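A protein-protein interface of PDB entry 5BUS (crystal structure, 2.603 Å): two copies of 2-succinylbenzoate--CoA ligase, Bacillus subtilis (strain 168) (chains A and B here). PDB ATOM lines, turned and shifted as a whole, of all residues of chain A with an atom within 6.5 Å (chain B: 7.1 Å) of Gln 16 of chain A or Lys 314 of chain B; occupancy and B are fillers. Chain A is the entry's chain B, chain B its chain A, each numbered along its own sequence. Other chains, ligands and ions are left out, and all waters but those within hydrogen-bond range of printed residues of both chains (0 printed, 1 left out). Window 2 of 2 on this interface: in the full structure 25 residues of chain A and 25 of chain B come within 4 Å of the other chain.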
ATOM      1  N   PRO A   8      10.655 -33.364  -1.488  1.00  0.00           N
ATOM      2  CA  PRO A   8       9.719 -32.281  -1.831  1.00  0.00           C
ATOM      3  C   PRO A   8      10.042 -31.675  -3.186  1.00  0.00           C
ATOM      4  O   PRO A   8      11.202 -31.581  -3.597  1.00  0.00           O
ATOM      5  CB  PRO A   8       9.895 -31.269  -0.694  1.00  0.00           C
ATOM      6  CG  PRO A   8      11.200 -31.678   0.013  1.00  0.00           C
ATOM      7  CD  PRO A   8      11.348 -33.143  -0.210  1.00  0.00           C
ATOM      8  N   LEU A  11      10.775 -27.071  -6.976  1.00  0.00           N
ATOM      9  CA  LEU A  11      10.348 -25.680  -7.151  1.00  0.00           C
ATOM     10  C   LEU A  11       9.683 -25.155  -5.900  1.00  0.00           C
ATOM     11  O   LEU A  11       9.935 -24.033  -5.475  1.00  0.00           O
ATOM     12  CB  LEU A  11       9.422 -25.546  -8.373  1.00  0.00           C
ATOM     13  CG  LEU A  11       8.764 -24.177  -8.597  1.00  0.00           C
ATOM     14  CD1 LEU A  11       9.777 -23.002  -8.752  1.00  0.00           C
ATOM     15  CD2 LEU A  11       7.865 -24.270  -9.808  1.00  0.00           C
ATOM     16  N   MET A  12       8.829 -25.981  -5.316  1.00  0.00           N
ATOM     17  CA  MET A  12       8.147 -25.607  -4.100  1.00  0.00           C
ATOM     18  C   MET A  12       9.167 -25.337  -2.989  1.00  0.00           C
ATOM     19  O   MET A  12       9.114 -24.290  -2.342  1.00  0.00           O
ATOM     20  CB  MET A  12       7.168 -26.695  -3.688  1.00  0.00           C
ATOM     21  CG  MET A  12       6.271 -26.346  -2.506  1.00  0.00           C
ATOM     22  SD  MET A  12       5.570 -27.882  -1.837  1.00  0.00           S
ATOM     23  CE  MET A  12       7.034 -28.601  -1.102  1.00  0.00           C
ATOM     24  N   GLN A  13      10.119 -26.247  -2.786  1.00  0.00           N
ATOM     25  CA  GLN A  13      11.067 -26.064  -1.687  1.00  0.00           C
ATOM     26  C   GLN A  13      11.967 -24.863  -1.967  1.00  0.00           C
ATOM     27  O   GLN A  13      12.242 -24.054  -1.072  1.00  0.00           O
ATOM     28  CB  GLN A  13      11.901 -27.333  -1.446  1.00  0.00           C
ATOM     29  CG  GLN A  13      12.965 -27.164  -0.395  1.00  0.00           C
ATOM     30  CD  GLN A  13      13.440 -28.471   0.242  1.00  0.00           C
ATOM     31  OE1 GLN A  13      13.734 -29.440  -0.442  1.00  0.00           O
ATOM     32  NE2 GLN A  13      13.543 -28.477   1.570  1.00  0.00           N
ATOM     33  N   ARG A  14      12.396 -24.735  -3.217  1.00  0.00           N
ATOM     34  CA  ARG A  14      13.254 -23.628  -3.614  1.00  0.00           C
ATOM     35  C   ARG A  14      12.546 -22.285  -3.385  1.00  0.00           C
ATOM     36  O   ARG A  14      13.156 -21.305  -2.917  1.00  0.00           O
ATOM     37  CB  ARG A  14      13.676 -23.778  -5.073  1.00  0.00           C
ATOM     38  CG  ARG A  14      14.430 -22.586  -5.631  1.00  0.00           C
ATOM     39  CD  ARG A  14      15.621 -22.208  -4.740  1.00  0.00           C
ATOM     40  NE  ARG A  14      16.537 -23.335  -4.506  1.00  0.00           N
ATOM     41  CZ  ARG A  14      17.495 -23.352  -3.575  1.00  0.00           C
ATOM     42  NH1 ARG A  14      18.283 -24.413  -3.442  1.00  0.00           N
ATOM     43  NH2 ARG A  14      17.676 -22.300  -2.785  1.00  0.00           N
ATOM     44  N   ALA A  15      11.252 -22.240  -3.684  1.00  0.00           N
ATOM     45  CA  ALA A  15      10.503 -21.007  -3.445  1.00  0.00           C
ATOM     46  C   ALA A  15      10.381 -20.762  -1.936  1.00  0.00           C
ATOM     47  O   ALA A  15      10.456 -19.626  -1.477  1.00  0.00           O
ATOM     48  CB  ALA A  15       9.136 -21.071  -4.093  1.00  0.00           C
ATOM     49  N   GLN A  16      10.198 -21.827  -1.164  1.00  0.00           N
ATOM     50  CA  GLN A  16      10.156 -21.682   0.278  1.00  0.00           C
ATOM     51  C   GLN A  16      11.474 -21.132   0.837  1.00  0.00           C
ATOM     52  O   GLN A  16      11.471 -20.222   1.661  1.00  0.00           O
ATOM     53  CB  GLN A  16       9.838 -23.011   0.930  1.00  0.00           C
ATOM     54  CG  GLN A  16       8.432 -23.490   0.728  1.00  0.00           C
ATOM     55  CD  GLN A  16       8.254 -24.886   1.285  1.00  0.00           C
ATOM     56  OE1 GLN A  16       9.222 -25.494   1.723  1.00  0.00           O
ATOM     57  NE2 GLN A  16       7.029 -25.413   1.243  1.00  0.00           N
ATOM     58  N   LEU A  17      12.596 -21.679   0.379  1.00  0.00           N
ATOM     59  CA  LEU A  17      13.899 -21.322   0.937  1.00  0.00           C
ATOM     60  C   LEU A  17      14.341 -19.934   0.553  1.00  0.00           C
ATOM     61  O   LEU A  17      14.562 -19.091   1.410  1.00  0.00           O
ATOM     62  CB  LEU A  17      14.959 -22.319   0.488  1.00  0.00           C
ATOM     63  CG  LEU A  17      14.732 -23.699   1.072  1.00  0.00           C
ATOM     64  CD1 LEU A  17      15.872 -24.607   0.653  1.00  0.00           C
ATOM     65  CD2 LEU A  17      14.572 -23.593   2.607  1.00  0.00           C
ATOM     66  N   THR A  18      14.497 -19.707  -0.745  1.00  0.00           N
ATOM     67  CA  THR A  18      14.953 -18.413  -1.229  1.00  0.00           C
ATOM     68  C   THR A  18      13.996 -17.844  -2.272  1.00  0.00           C
ATOM     69  O   THR A  18      14.273 -17.861  -3.465  1.00  0.00           O
ATOM     70  CB  THR A  18      16.360 -18.512  -1.807  1.00  0.00           C
ATOM     71  OG1 THR A  18      16.345 -19.352  -2.966  1.00  0.00           O
ATOM     72  CG2 THR A  18      17.321 -19.094  -0.753  1.00  0.00           C
ATOM     73  N   PRO A  19      12.869 -17.305  -1.798  1.00  0.00           N
ATOM     74  CA  PRO A  19      11.739 -16.769  -2.560  1.00  0.00           C
ATOM     75  C   PRO A  19      12.088 -15.698  -3.601  1.00  0.00           C
ATOM     76  O   PRO A  19      11.405 -15.610  -4.622  1.00  0.00           O
ATOM     77  CB  PRO A  19      10.853 -16.145  -1.468  1.00  0.00           C
ATOM     78  CG  PRO A  19      11.224 -16.827  -0.232  1.00  0.00           C
ATOM     79  CD  PRO A  19      12.683 -17.111  -0.352  1.00  0.00           C
ATOM     80  N   PHE A  33      11.901 -17.201  -7.829  1.00  0.00           N
ATOM     81  CA  PHE A  33      11.429 -18.550  -7.573  1.00  0.00           C
ATOM     82  C   PHE A  33      10.019 -18.534  -6.987  1.00  0.00           C
ATOM     83  O   PHE A  33       9.191 -19.392  -7.310  1.00  0.00           O
ATOM     84  CB  PHE A  33      12.417 -19.304  -6.675  1.00  0.00           C
ATOM     85  CG  PHE A  33      13.680 -19.671  -7.382  1.00  0.00           C
ATOM     86  CD1 PHE A  33      13.699 -20.739  -8.273  1.00  0.00           C
ATOM     87  CD2 PHE A  33      14.844 -18.953  -7.179  1.00  0.00           C
ATOM     88  CE1 PHE A  33      14.855 -21.085  -8.945  1.00  0.00           C
ATOM     89  CE2 PHE A  33      16.013 -19.304  -7.847  1.00  0.00           C
ATOM     90  CZ  PHE A  33      16.014 -20.365  -8.731  1.00  0.00           C
ATOM     91  N   ASN B 181      23.495 -25.897   0.299  1.00  0.00           N
ATOM     92  CA  ASN B 181      23.237 -24.828   1.254  1.00  0.00           C
ATOM     93  C   ASN B 181      24.418 -23.848   1.225  1.00  0.00           C
ATOM     94  O   ASN B 181      24.218 -22.649   1.233  1.00  0.00           O
ATOM     95  CB  ASN B 181      23.025 -25.411   2.671  1.00  0.00           C
ATOM     96  CG  ASN B 181      22.678 -24.350   3.725  1.00  0.00           C
ATOM     97  OD1 ASN B 181      23.239 -24.331   4.808  1.00  0.00           O
ATOM     98  ND2 ASN B 181      21.742 -23.480   3.404  1.00  0.00           N
ATOM     99  N   GLN B 286      24.455 -20.569  11.923  1.00  0.00           N
ATOM    100  CA  GLN B 286      23.886 -21.380  12.978  1.00  0.00           C
ATOM    101  C   GLN B 286      23.162 -22.596  12.363  1.00  0.00           C
ATOM    102  O   GLN B 286      22.736 -22.588  11.191  1.00  0.00           O
ATOM    103  CB  GLN B 286      22.971 -20.535  13.856  1.00  0.00           C
ATOM    104  CG  GLN B 286      23.749 -19.400  14.502  1.00  0.00           C
ATOM    105  CD  GLN B 286      22.857 -18.458  15.240  1.00  0.00           C
ATOM    106  OE1 GLN B 286      22.509 -18.692  16.405  1.00  0.00           O
ATOM    107  NE2 GLN B 286      22.441 -17.387  14.559  1.00  0.00           N
ATOM    108  N   ILE B 297      20.713 -30.438   9.672  1.00  0.00           N
ATOM    109  CA  ILE B 297      19.565 -30.581   8.798  1.00  0.00           C
ATOM    110  C   ILE B 297      18.869 -29.216   8.613  1.00  0.00           C
ATOM    111  O   ILE B 297      18.151 -29.006   7.640  1.00  0.00           O
ATOM    112  CB  ILE B 297      18.606 -31.667   9.350  1.00  0.00           C
ATOM    113  CG1 ILE B 297      17.498 -32.004   8.344  1.00  0.00           C
ATOM    114  CG2 ILE B 297      18.083 -31.299  10.757  1.00  0.00           C
ATOM    115  CD1 ILE B 297      16.613 -33.143   8.804  1.00  0.00           C
ATOM    116  N   VAL B 298      19.137 -28.277   9.521  1.00  0.00           N
ATOM    117  CA  VAL B 298      18.579 -26.925   9.436  1.00  0.00           C
ATOM    118  C   VAL B 298      19.692 -25.892   9.609  1.00  0.00           C
ATOM    119  O   VAL B 298      20.536 -26.056  10.497  1.00  0.00           O
ATOM    120  CB  VAL B 298      17.492 -26.684  10.519  1.00  0.00           C
ATOM    121  CG1 VAL B 298      17.087 -25.210  10.575  1.00  0.00           C
ATOM    122  CG2 VAL B 298      16.271 -27.580  10.280  1.00  0.00           C
ATOM    123  N   THR B 299      19.732 -24.845   8.778  1.00  0.00           N
ATOM    124  CA  THR B 299      20.758 -23.823   8.989  1.00  0.00           C
ATOM    125  C   THR B 299      20.233 -22.401   8.852  1.00  0.00           C
ATOM    126  O   THR B 299      19.201 -22.153   8.224  1.00  0.00           O
ATOM    127  CB  THR B 299      21.975 -23.977   8.025  1.00  0.00           C
ATOM    128  OG1 THR B 299      21.595 -23.720   6.674  1.00  0.00           O
ATOM    129  CG2 THR B 299      22.590 -25.362   8.138  1.00  0.00           C
ATOM    130  N   LEU B 300      20.948 -21.469   9.471  1.00  0.00           N
ATOM    131  CA  LEU B 300      20.627 -20.039   9.366  1.00  0.00           C
ATOM    132  C   LEU B 300      21.808 -19.265   8.773  1.00  0.00           C
ATOM    133  O   LEU B 300      22.921 -19.333   9.280  1.00  0.00           O
ATOM    134  CB  LEU B 300      20.255 -19.474  10.730  1.00  0.00           C
ATOM    135  CG  LEU B 300      19.774 -18.032  10.665  1.00  0.00           C
ATOM    136  CD1 LEU B 300      18.340 -18.041  10.193  1.00  0.00           C
ATOM    137  CD2 LEU B 300      19.911 -17.341  12.018  1.00  0.00           C
ATOM    138  N   SER B 301      21.576 -18.551   7.683  1.00  0.00           N
ATOM    139  CA  SER B 301      22.668 -17.860   7.005  1.00  0.00           C
ATOM    140  C   SER B 301      23.059 -16.619   7.840  1.00  0.00           C
ATOM    141  O   SER B 301      22.243 -16.125   8.614  1.00  0.00           O
ATOM    142  CB  SER B 301      22.255 -17.510   5.557  1.00  0.00           C
ATOM    143  N   PHE B 304      21.048 -13.407   8.440  1.00  0.00           N
ATOM    144  CA  PHE B 304      19.818 -13.470   9.222  1.00  0.00           C
ATOM    145  C   PHE B 304      20.143 -13.540  10.700  1.00  0.00           C
ATOM    146  O   PHE B 304      19.242 -13.584  11.543  1.00  0.00           O
ATOM    147  CB  PHE B 304      18.936 -14.667   8.823  1.00  0.00           C
ATOM    148  CG  PHE B 304      18.404 -14.599   7.412  1.00  0.00           C
ATOM    149  CD1 PHE B 304      17.306 -13.805   7.108  1.00  0.00           C
ATOM    150  CD2 PHE B 304      18.951 -15.385   6.408  1.00  0.00           C
ATOM    151  CE1 PHE B 304      16.801 -13.753   5.821  1.00  0.00           C
ATOM    152  CE2 PHE B 304      18.439 -15.349   5.124  1.00  0.00           C
ATOM    153  CZ  PHE B 304      17.366 -14.530   4.831  1.00  0.00           C
ATOM    154  N   SER B 311      16.916 -18.268  16.226  1.00  0.00           N
ATOM    155  CA  SER B 311      16.491 -19.263  15.231  1.00  0.00           C
ATOM    156  C   SER B 311      17.635 -20.130  14.703  1.00  0.00           C
ATOM    157  O   SER B 311      18.738 -19.645  14.480  1.00  0.00           O
ATOM    158  CB  SER B 311      15.820 -18.593  14.030  1.00  0.00           C
ATOM    159  OG  SER B 311      15.522 -19.560  13.021  1.00  0.00           O
ATOM    160  N   ALA B 312      17.346 -21.404  14.464  1.00  0.00           N
ATOM    161  CA  ALA B 312      18.324 -22.317  13.875  1.00  0.00           C
ATOM    162  C   ALA B 312      18.263 -22.242  12.355  1.00  0.00           C
ATOM    163  O   ALA B 312      19.098 -22.823  11.667  1.00  0.00           O
ATOM    164  CB  ALA B 312      18.079 -23.751  14.347  1.00  0.00           C
ATOM    165  N   GLY B 313      17.267 -21.531  11.836  1.00  0.00           N
ATOM    166  CA  GLY B 313      17.151 -21.333  10.403  1.00  0.00           C
ATOM    167  C   GLY B 313      16.099 -22.165   9.688  1.00  0.00           C
ATOM    168  O   GLY B 313      15.010 -22.453  10.211  1.00  0.00           O
ATOM    169  N   LYS B 314      16.448 -22.583   8.482  1.00  0.00           N
ATOM    170  CA  LYS B 314      15.518 -23.322   7.636  1.00  0.00           C
ATOM    171  C   LYS B 314      16.121 -24.655   7.198  1.00  0.00           C
ATOM    172  O   LYS B 314      17.326 -24.829   7.259  1.00  0.00           O
ATOM    173  CB  LYS B 314      15.136 -22.469   6.436  1.00  0.00           C
ATOM    174  CG  LYS B 314      14.018 -21.476   6.713  1.00  0.00           C
ATOM    175  CD  LYS B 314      13.830 -20.617   5.493  1.00  0.00           C
ATOM    176  CE  LYS B 314      12.671 -19.649   5.596  1.00  0.00           C
ATOM    177  NZ  LYS B 314      12.735 -18.724   4.418  1.00  0.00           N
ATOM    178  N   PRO B 315      15.280 -25.615   6.781  1.00  0.00           N
ATOM    179  CA  PRO B 315      15.820 -26.943   6.449  1.00  0.00           C
ATOM    180  C   PRO B 315      16.753 -26.900   5.235  1.00  0.00           C
ATOM    181  O   PRO B 315      16.508 -26.114   4.311  1.00  0.00           O
ATOM    182  CB  PRO B 315      14.573 -27.756   6.071  1.00  0.00           C
ATOM    183  CG  PRO B 315      13.371 -26.902   6.410  1.00  0.00           C
ATOM    184  CD  PRO B 315      13.847 -25.493   6.441  1.00  0.00           C
ATOM    185  N   LEU B 316      17.766 -27.762   5.204  1.00  0.00           N
ATOM    186  CA  LEU B 316      18.554 -27.951   3.984  1.00  0.00           C
ATOM    187  C   LEU B 316      17.689 -28.462   2.839  1.00  0.00           C
ATOM    188  O   LEU B 316      16.591 -29.015   3.047  1.00  0.00           O
ATOM    189  CB  LEU B 316      19.723 -28.925   4.220  1.00  0.00           C
ATOM    190  CG  LEU B 316      20.706 -28.516   5.328  1.00  0.00           C
ATOM    191  CD1 LEU B 316      21.923 -29.390   5.309  1.00  0.00           C
ATOM    192  CD2 LEU B 316      21.117 -27.066   5.179  1.00  0.00           C
ATOM    193  N   PHE B 317      18.192 -28.300   1.623  1.00  0.00           N
ATOM    194  CA  PHE B 317      17.443 -28.762   0.470  1.00  0.00           C
ATOM    195  C   PHE B 317      17.247 -30.276   0.591  1.00  0.00           C
ATOM    196  O   PHE B 317      18.087 -30.956   1.171  1.00  0.00           O
ATOM    197  CB  PHE B 317      18.155 -28.395  -0.820  1.00  0.00           C
ATOM    198  CG  PHE B 317      17.244 -28.292  -1.988  1.00  0.00           C
ATOM    199  CD1 PHE B 317      16.546 -27.120  -2.222  1.00  0.00           C
ATOM    200  CD2 PHE B 317      17.069 -29.372  -2.850  1.00  0.00           C
ATOM    201  CE1 PHE B 317      15.683 -27.014  -3.294  1.00  0.00           C
ATOM    202  CE2 PHE B 317      16.216 -29.274  -3.930  1.00  0.00           C
ATOM    203  CZ  PHE B 317      15.517 -28.088  -4.158  1.00  0.00           C
ATOM    204  N   CYS B 319      15.172 -31.622   2.585  1.00  0.00           N
ATOM    205  CA  CYS B 319      14.867 -31.990   3.971  1.00  0.00           C
ATOM    206  C   CYS B 319      13.640 -31.276   4.444  1.00  0.00           C
ATOM    207  O   CYS B 319      13.243 -30.262   3.862  1.00  0.00           O
ATOM    208  CB  CYS B 319      16.036 -31.661   4.917  1.00  0.00           C
ATOM    209  SG  CYS B 319      17.622 -32.376   4.476  1.00  0.00           S
ATOM    210  N   ILE B 321      11.128 -30.147   8.066  1.00  0.00           N
ATOM    211  CA  ILE B 321      10.826 -30.109   9.485  1.00  0.00           C
ATOM    212  C   ILE B 321       9.364 -29.774   9.667  1.00  0.00           C
ATOM    213  O   ILE B 321       8.743 -29.180   8.793  1.00  0.00           O
ATOM    214  CB  ILE B 321      11.643 -29.050  10.259  1.00  0.00           C
ATOM    215  CG1 ILE B 321      11.468 -27.701   9.603  1.00  0.00           C
ATOM    216  CG2 ILE B 321      13.108 -29.424  10.336  1.00  0.00           C
ATOM    217  CD1 ILE B 321      12.162 -26.576  10.333  1.00  0.00           C
ATOM    218  N   ASP B 374       8.184 -19.827  13.261  1.00  0.00           N
ATOM    219  CA  ASP B 374       7.520 -18.537  13.079  1.00  0.00           C
ATOM    220  C   ASP B 374       6.832 -18.547  11.713  1.00  0.00           C
ATOM    221  O   ASP B 374       6.936 -19.521  10.969  1.00  0.00           O
ATOM    222  CB  ASP B 374       8.510 -17.366  13.238  1.00  0.00           C
ATOM    223  CG  ASP B 374       9.511 -17.239  12.083  1.00  0.00           C
ATOM    224  OD1 ASP B 374       9.322 -17.828  10.998  1.00  0.00           O
ATOM    225  OD2 ASP B 374      10.531 -16.541  12.272  1.00  0.00           O
ATOM    226  N   GLU B 376       7.347 -17.346   8.878  1.00  0.00           N
ATOM    227  CA  GLU B 376       8.142 -17.481   7.659  1.00  0.00           C
ATOM    228  C   GLU B 376       8.774 -18.872   7.580  1.00  0.00           C
ATOM    229  O   GLU B 376       9.475 -19.192   6.624  1.00  0.00           O
ATOM    230  CB  GLU B 376       9.228 -16.411   7.607  1.00  0.00           C
ATOM    231  CG  GLU B 376       8.828 -15.118   6.905  1.00  0.00           C
ATOM    232  CD  GLU B 376      10.009 -14.167   6.749  1.00  0.00           C
ATOM    233  OE1 GLU B 376      10.199 -13.609   5.650  1.00  0.00           O
ATOM    234  OE2 GLU B 376      10.761 -13.989   7.731  1.00  0.00           O
ATOM    235  N   GLY B 377       8.556 -19.685   8.610  1.00  0.00           N
ATOM    236  CA  GLY B 377       9.099 -21.028   8.630  1.00  0.00           C
ATOM    237  C   GLY B 377      10.470 -21.170   9.260  1.00  0.00           C
ATOM    238  O   GLY B 377      11.104 -22.210   9.134  1.00  0.00           O
ATOM    239  N   PHE B 378      10.949 -20.148   9.948  1.00  0.00           N
ATOM    240  CA  PHE B 378      12.202 -20.332  10.657  1.00  0.00           C
ATOM    241  C   PHE B 378      11.959 -21.128  11.920  1.00  0.00           C
ATOM    242  O   PHE B 378      10.917 -20.979  12.575  1.00  0.00           O
ATOM    243  CB  PHE B 378      12.861 -19.002  10.978  1.00  0.00           C
ATOM    244  CG  PHE B 378      13.358 -18.280   9.763  1.00  0.00           C
ATOM    245  CD1 PHE B 378      12.494 -17.527   8.988  1.00  0.00           C
ATOM    246  CD2 PHE B 378      14.690 -18.372   9.385  1.00  0.00           C
ATOM    247  CE1 PHE B 378      12.956 -16.864   7.859  1.00  0.00           C
ATOM    248  CE2 PHE B 378      15.159 -17.706   8.270  1.00  0.00           C
ATOM    249  CZ  PHE B 378      14.284 -16.951   7.500  1.00  0.00           C
ATOM    250  N   LEU B 379      12.925 -21.984  12.246  1.00  0.00           N
ATOM    251  CA  LEU B 379      12.837 -22.862  13.410  1.00  0.00           C
ATOM    252  C   LEU B 379      13.486 -22.255  14.672  1.00  0.00           C
ATOM    253  O   LEU B 379      14.580 -21.676  14.614  1.00  0.00           O
ATOM    254  CB  LEU B 379      13.491 -24.207  13.074  1.00  0.00           C
ATOM    255  CG  LEU B 379      13.720 -25.183  14.225  1.00  0.00           C
ATOM    256  CD1 LEU B 379      12.391 -25.762  14.646  1.00  0.00           C
ATOM    257  CD2 LEU B 379      14.675 -26.285  13.802  1.00  0.00           C
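Of the 22 printed residues of chain B, 5 touch a printed residue of chain A.
Hydrophobic or aromatic side chains of chain B that line the printed part of chain A: Phe 317.
Of the 11 printed residues of chain A, 4 touch a printed residue of chain B.
Hydrophobic or aromatic side chains of chain A that line the printed part of chain B: Leu 17.
Among the printed residues, 8 pairs touch across the chains.
Among the printed residues, no Asp or Glu carboxylate lies within 4 Å of a Lys or Arg side-chain nitrogen of the other chain.
The side-chain amino group (NZ) of Lys 314 of chain B lies within hydrogen-bond range of the backbone carbonyl oxygen (O) of Gln 16 of chain A (3.4 Å).
The backbone carbonyl oxygen (O) of Leu 316 of chain B is in hydrogen-bond range of the side-chain amide nitrogen (NE2) of Gln 13 of chain A (3.4 Å).
O of Cys 319 of chain B lies within hydrogen-bond range of NE2 of Gln 13 of chain A, at 2.9 Å.
No position is printed for both chains.
Gln 13 of chain A touches Phe 317 of chain B.
CD1 of Phe 317 of chain B touches NH1 of Arg 14 of chain A, 3.4 Å away.
Leu 17 of chain A touches Lys 314 of chain B.
Leu 17 of chain A touches Pro 315 of chain B.
CD1 of Phe 317 of chain B touches CD1 of Leu 17 of chain A, at 3.9 Å.
Gln 16 of chain A touches just one residue of chain B: Lys 314.
Phe 304 of chain B touches none of the printed residues of chain A.
Of the printed residues of chain A, Lys 314 of chain B touches Gln 16 and Leu 17.
Printed residues of chain A within 4 Å of Leu 316 of chain B: Gln 13 (3.4 Å).
Printed residues of chain A within 4 Å of Phe 317 of chain B: Gln 13, Arg 14 and Leu 17.
Ile 321 of chain B touches none of the printed residues of chain A.
The nearest residue of chain A that does not touch Lys 314 of chain B is Pro 19 of chain A (5.0 Å).
The backbone carbonyl oxygen (O) of Ile 297 of chain B lies within hydrogen-bond range of the backbone NH (N) of Leu 316 of chain B (2.8 Å).
The backbone carbonyl oxygen (O) of Thr 299 of chain B sits at hydrogen-bond distance from the backbone NH (N) of Lys 314 of chain B (2.8 Å).
O of Leu 316 of chain B lies close to SG of Cys 319 of chain B (3.8 Å).
O of Phe 317 of chain B sits at hydrogen-bond distance from SG of Cys 319 of chain B.
The side-chain hydroxyl (OG1) of Thr 18 of chain A lies within hydrogen-bond range of the guanidinium group (NH2) of Arg 14 of chain A.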
